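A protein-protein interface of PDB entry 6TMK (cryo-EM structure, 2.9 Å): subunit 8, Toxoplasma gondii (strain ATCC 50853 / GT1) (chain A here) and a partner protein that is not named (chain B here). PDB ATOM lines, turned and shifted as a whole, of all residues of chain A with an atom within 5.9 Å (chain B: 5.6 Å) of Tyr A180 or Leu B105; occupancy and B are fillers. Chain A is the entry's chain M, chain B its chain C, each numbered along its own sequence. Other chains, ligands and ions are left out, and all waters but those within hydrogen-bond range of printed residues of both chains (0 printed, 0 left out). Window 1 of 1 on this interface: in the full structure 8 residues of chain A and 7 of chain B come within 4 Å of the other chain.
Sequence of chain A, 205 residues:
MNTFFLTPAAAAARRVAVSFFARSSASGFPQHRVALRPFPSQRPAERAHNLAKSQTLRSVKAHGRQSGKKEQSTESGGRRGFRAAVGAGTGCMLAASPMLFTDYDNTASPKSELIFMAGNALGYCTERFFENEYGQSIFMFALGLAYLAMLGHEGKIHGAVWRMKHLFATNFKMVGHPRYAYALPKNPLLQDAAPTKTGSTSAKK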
ATOM      1  N   HIS A 177     -13.003 -13.274 -10.320  1.00  0.00           N
ATOM      2  CA  HIS A 177     -12.627 -12.947  -8.960  1.00  0.00           C
ATOM      3  C   HIS A 177     -13.656 -13.513  -7.986  1.00  0.00           C
ATOM      4  O   HIS A 177     -14.848 -13.562  -8.298  1.00  0.00           O
ATOM      5  CB  HIS A 177     -12.517 -11.440  -8.783  1.00  0.00           C
ATOM      6  CG  HIS A 177     -11.782 -11.035  -7.548  1.00  0.00           C
ATOM      7  ND1 HIS A 177     -12.420 -10.557  -6.425  1.00  0.00           N
ATOM      8  CD2 HIS A 177     -10.462 -11.049  -7.253  1.00  0.00           C
ATOM      9  CE1 HIS A 177     -11.523 -10.291  -5.493  1.00  0.00           C
ATOM     10  NE2 HIS A 177     -10.328 -10.580  -5.971  1.00  0.00           N
ATOM     11  N   PRO A 178     -13.248 -13.964  -6.796  1.00  0.00           N
ATOM     12  CA  PRO A 178     -14.223 -14.600  -5.900  1.00  0.00           C
ATOM     13  C   PRO A 178     -15.286 -13.653  -5.381  1.00  0.00           C
ATOM     14  O   PRO A 178     -16.357 -14.120  -4.972  1.00  0.00           O
ATOM     15  CB  PRO A 178     -13.353 -15.139  -4.758  1.00  0.00           C
ATOM     16  CG  PRO A 178     -11.957 -15.101  -5.272  1.00  0.00           C
ATOM     17  CD  PRO A 178     -11.901 -13.966  -6.211  1.00  0.00           C
ATOM     18  N   ARG A 179     -15.035 -12.345  -5.375  1.00  0.00           N
ATOM     19  CA  ARG A 179     -16.026 -11.401  -4.878  1.00  0.00           C
ATOM     20  C   ARG A 179     -17.250 -11.314  -5.773  1.00  0.00           C
ATOM     21  O   ARG A 179     -18.267 -10.754  -5.349  1.00  0.00           O
ATOM     22  CB  ARG A 179     -15.410 -10.013  -4.731  1.00  0.00           C
ATOM     23  CG  ARG A 179     -14.689  -9.783  -3.424  1.00  0.00           C
ATOM     24  CD  ARG A 179     -14.024  -8.425  -3.404  1.00  0.00           C
ATOM     25  NE  ARG A 179     -15.001  -7.340  -3.381  1.00  0.00           N
ATOM     26  CZ  ARG A 179     -15.471  -6.770  -2.275  1.00  0.00           C
ATOM     27  NH1 ARG A 179     -15.063  -7.171  -1.080  1.00  0.00           N
ATOM     28  NH2 ARG A 179     -16.360  -5.793  -2.367  1.00  0.00           N
ATOM     29  N   TYR A 180     -17.177 -11.846  -6.993  1.00  0.00           N
ATOM     30  CA  TYR A 180     -18.267 -11.772  -7.956  1.00  0.00           C
ATOM     31  C   TYR A 180     -18.800 -13.149  -8.327  1.00  0.00           C
ATOM     32  O   TYR A 180     -19.442 -13.303  -9.369  1.00  0.00           O
ATOM     33  CB  TYR A 180     -17.809 -11.016  -9.199  1.00  0.00           C
ATOM     34  CG  TYR A 180     -17.264  -9.650  -8.880  1.00  0.00           C
ATOM     35  CD1 TYR A 180     -18.097  -8.549  -8.831  1.00  0.00           C
ATOM     36  CD2 TYR A 180     -15.922  -9.467  -8.611  1.00  0.00           C
ATOM     37  CE1 TYR A 180     -17.608  -7.304  -8.534  1.00  0.00           C
ATOM     38  CE2 TYR A 180     -15.423  -8.227  -8.310  1.00  0.00           C
ATOM     39  CZ  TYR A 180     -16.271  -7.147  -8.271  1.00  0.00           C
ATOM     40  OH  TYR A 180     -15.776  -5.901  -7.972  1.00  0.00           O
ATOM     41  N   ALA A 181     -18.545 -14.152  -7.491  1.00  0.00           N
ATOM     42  CA  ALA A 181     -18.995 -15.506  -7.768  1.00  0.00           C
ATOM     43  C   ALA A 181     -20.500 -15.663  -7.617  1.00  0.00           C
ATOM     44  O   ALA A 181     -21.047 -16.676  -8.064  1.00  0.00           O
ATOM     45  CB  ALA A 181     -18.275 -16.482  -6.847  1.00  0.00           C
ATOM     46  N   TYR A 182     -21.177 -14.697  -6.995  1.00  0.00           N
ATOM     47  CA  TYR A 182     -22.630 -14.745  -6.919  1.00  0.00           C
ATOM     48  C   TYR A 182     -23.261 -14.719  -8.301  1.00  0.00           C
ATOM     49  O   TYR A 182     -24.334 -15.296  -8.505  1.00  0.00           O
ATOM     50  CB  TYR A 182     -23.156 -13.572  -6.092  1.00  0.00           C
ATOM     51  CG  TYR A 182     -22.849 -12.214  -6.675  1.00  0.00           C
ATOM     52  CD1 TYR A 182     -23.714 -11.616  -7.580  1.00  0.00           C
ATOM     53  CD2 TYR A 182     -21.707 -11.522  -6.314  1.00  0.00           C
ATOM     54  CE1 TYR A 182     -23.441 -10.376  -8.115  1.00  0.00           C
ATOM     55  CE2 TYR A 182     -21.429 -10.282  -6.845  1.00  0.00           C
ATOM     56  CZ  TYR A 182     -22.299  -9.715  -7.744  1.00  0.00           C
ATOM     57  OH  TYR A 182     -22.024  -8.477  -8.274  1.00  0.00           O
ATOM     58  N   ALA A 183     -22.613 -14.060  -9.258  1.00  0.00           N
ATOM     59  CA  ALA A 183     -23.183 -13.881 -10.583  1.00  0.00           C
ATOM     60  C   ALA A 183     -23.005 -15.093 -11.479  1.00  0.00           C
ATOM     61  O   ALA A 183     -23.619 -15.143 -12.550  1.00  0.00           O
ATOM     62  CB  ALA A 183     -22.555 -12.661 -11.251  1.00  0.00           C
ATOM     63  N   LEU A 184     -22.193 -16.063 -11.080  1.00  0.00           N
ATOM     64  CA  LEU A 184     -21.976 -17.229 -11.910  1.00  0.00           C
ATOM     65  C   LEU A 184     -23.230 -18.092 -11.961  1.00  0.00           C
ATOM     66  O   LEU A 184     -24.082 -18.024 -11.072  1.00  0.00           O
ATOM     67  CB  LEU A 184     -20.811 -18.055 -11.384  1.00  0.00           C
ATOM     68  CG  LEU A 184     -19.411 -17.559 -11.721  1.00  0.00           C
ATOM     69  CD1 LEU A 184     -18.378 -18.446 -11.085  1.00  0.00           C
ATOM     70  CD2 LEU A 184     -19.220 -17.526 -13.220  1.00  0.00           C
ATOM     71  N   GLN B 102     -19.464  -0.797 -14.325  1.00  0.00           N
ATOM     72  CA  GLN B 102     -19.580  -1.368 -12.990  1.00  0.00           C
ATOM     73  C   GLN B 102     -19.743  -2.882 -13.029  1.00  0.00           C
ATOM     74  O   GLN B 102     -19.154  -3.592 -12.205  1.00  0.00           O
ATOM     75  CB  GLN B 102     -20.764  -0.738 -12.264  1.00  0.00           C
ATOM     76  CG  GLN B 102     -20.601   0.723 -11.937  1.00  0.00           C
ATOM     77  CD  GLN B 102     -21.921   1.412 -11.689  1.00  0.00           C
ATOM     78  OE1 GLN B 102     -22.961   0.766 -11.586  1.00  0.00           O
ATOM     79  NE2 GLN B 102     -21.887   2.730 -11.581  1.00  0.00           N
ATOM     80  N   GLN B 103     -20.542  -3.394 -13.962  1.00  0.00           N
ATOM     81  CA  GLN B 103     -20.935  -4.798 -13.980  1.00  0.00           C
ATOM     82  C   GLN B 103     -19.999  -5.679 -14.805  1.00  0.00           C
ATOM     83  O   GLN B 103     -20.345  -6.832 -15.103  1.00  0.00           O
ATOM     84  CB  GLN B 103     -22.366  -4.919 -14.504  1.00  0.00           C
ATOM     85  CG  GLN B 103     -23.374  -4.114 -13.712  1.00  0.00           C
ATOM     86  CD  GLN B 103     -23.418  -4.514 -12.254  1.00  0.00           C
ATOM     87  OE1 GLN B 103     -23.089  -5.644 -11.900  1.00  0.00           O
ATOM     88  NE2 GLN B 103     -23.831  -3.589 -11.400  1.00  0.00           N
ATOM     89  N   ARG B 104     -18.817  -5.172 -15.150  1.00  0.00           N
ATOM     90  CA  ARG B 104     -17.899  -5.907 -16.012  1.00  0.00           C
ATOM     91  C   ARG B 104     -17.413  -7.186 -15.344  1.00  0.00           C
ATOM     92  O   ARG B 104     -17.424  -8.261 -15.951  1.00  0.00           O
ATOM     93  CB  ARG B 104     -16.721  -5.013 -16.375  1.00  0.00           C
ATOM     94  CG  ARG B 104     -17.028  -3.966 -17.406  1.00  0.00           C
ATOM     95  CD  ARG B 104     -15.778  -3.519 -18.095  1.00  0.00           C
ATOM     96  NE  ARG B 104     -15.884  -2.188 -18.676  1.00  0.00           N
ATOM     97  CZ  ARG B 104     -16.593  -1.892 -19.756  1.00  0.00           C
ATOM     98  NH1 ARG B 104     -17.278  -2.828 -20.385  1.00  0.00           N
ATOM     99  NH2 ARG B 104     -16.622  -0.653 -20.207  1.00  0.00           N
ATOM    100  N   LEU B 105     -16.973  -7.085 -14.093  1.00  0.00           N
ATOM    101  CA  LEU B 105     -16.422  -8.229 -13.382  1.00  0.00           C
ATOM    102  C   LEU B 105     -17.483  -9.215 -12.929  1.00  0.00           C
ATOM    103  O   LEU B 105     -17.135 -10.319 -12.501  1.00  0.00           O
ATOM    104  CB  LEU B 105     -15.618  -7.759 -12.178  1.00  0.00           C
ATOM    105  CG  LEU B 105     -14.128  -7.511 -12.387  1.00  0.00           C
ATOM    106  CD1 LEU B 105     -13.885  -6.597 -13.535  1.00  0.00           C
ATOM    107  CD2 LEU B 105     -13.539  -6.925 -11.138  1.00  0.00           C
ATOM    108  N   ALA B 106     -18.756  -8.846 -13.005  1.00  0.00           N
ATOM    109  CA  ALA B 106     -19.837  -9.750 -12.657  1.00  0.00           C
ATOM    110  C   ALA B 106     -20.474 -10.412 -13.866  1.00  0.00           C
ATOM    111  O   ALA B 106     -21.091 -11.471 -13.714  1.00  0.00           O
ATOM    112  CB  ALA B 106     -20.918  -9.001 -11.878  1.00  0.00           C
ATOM    113  N   ARG B 107     -20.342  -9.826 -15.054  1.00  0.00           N
ATOM    114  CA  ARG B 107     -20.965 -10.426 -16.228  1.00  0.00           C
ATOM    115  C   ARG B 107     -20.300 -11.749 -16.608  1.00  0.00           C
ATOM    116  O   ARG B 107     -20.986 -12.737 -16.899  1.00  0.00           O
ATOM    117  CB  ARG B 107     -20.917  -9.438 -17.389  1.00  0.00           C
ATOM    118  CG  ARG B 107     -22.070  -8.462 -17.393  1.00  0.00           C
ATOM    119  CD  ARG B 107     -22.047  -7.549 -18.598  1.00  0.00           C
ATOM    120  NE  ARG B 107     -21.475  -6.242 -18.288  1.00  0.00           N
ATOM    121  CZ  ARG B 107     -20.826  -5.478 -19.164  1.00  0.00           C
ATOM    122  NH1 ARG B 107     -20.660  -5.873 -20.418  1.00  0.00           N
ATOM    123  NH2 ARG B 107     -20.344  -4.308 -18.780  1.00  0.00           N
ATOM    124  N   HIS B 108     -18.968 -11.775 -16.644  1.00  0.00           N
ATOM    125  CA  HIS B 108     -18.163 -12.983 -16.852  1.00  0.00           C
ATOM    126  C   HIS B 108     -18.205 -13.504 -18.282  1.00  0.00           C
ATOM    127  O   HIS B 108     -17.430 -14.400 -18.628  1.00  0.00           O
ATOM    128  CB  HIS B 108     -18.599 -14.153 -15.959  1.00  0.00           C
ATOM    129  CG  HIS B 108     -18.282 -13.997 -14.508  1.00  0.00           C
ATOM    130  ND1 HIS B 108     -19.174 -13.478 -13.598  1.00  0.00           N
ATOM    131  CD2 HIS B 108     -17.183 -14.347 -13.799  1.00  0.00           C
ATOM    132  CE1 HIS B 108     -18.629 -13.488 -12.395  1.00  0.00           C
ATOM    133  NE2 HIS B 108     -17.422 -14.013 -12.490  1.00  0.00           N
ATOM    134  N   PRO B 111     -17.635  -8.970 -20.582  1.00  0.00           N
ATOM    135  CA  PRO B 111     -17.102  -7.796 -19.885  1.00  0.00           C
ATOM    136  C   PRO B 111     -16.996  -6.590 -20.789  1.00  0.00           C
ATOM    137  O   PRO B 111     -17.140  -5.454 -20.320  1.00  0.00           O
ATOM    138  CB  PRO B 111     -15.726  -8.269 -19.401  1.00  0.00           C
ATOM    139  CG  PRO B 111     -15.767  -9.738 -19.471  1.00  0.00           C
ATOM    140  CD  PRO B 111     -16.693 -10.094 -20.563  1.00  0.00           C
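A ring nitrogen (ND1) of His B108 lies within hydrogen-bond range of the backbone carbonyl oxygen (O) of Ala B106 (2.8 Å).
Tyr A180 touches Leu B105.
Tyr A180 touches His B108.
OH of Tyr A182 touches CB of Ala B106, at 3.8 Å.
O of Ala B106 touches CB of Ala A183, 3.1 Å away.
Leu A184 touches His B108 (CD2 to CD2, 3.8 Å).
Of chain A, only Tyr A180 (3.4 Å) comes within 4 Å of Leu B105.
Printed residues of chain A within 4 Å of His B108: Tyr A180 (3.1 Å) and Leu A184 (3.8 Å).
Printed residues of chain B within 4 Å of Leu A184: His B108.
The nearest residue of chain B that does not touch Tyr A180 is Ala B106 (4.2 Å).
Of the 8 printed residues of chain A, 4 touch a printed residue of chain B.
Hydrophobic or aromatic side chains of chain A within 4 Å of the printed part of chain B: Tyr A180, Tyr A182, Ala A183 and Leu A184.
Printed residues of chain B that touch a printed residue of chain A: Leu B105, Ala B106 and His B108.
Among the printed residues, 5 pairs touch across the chains.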
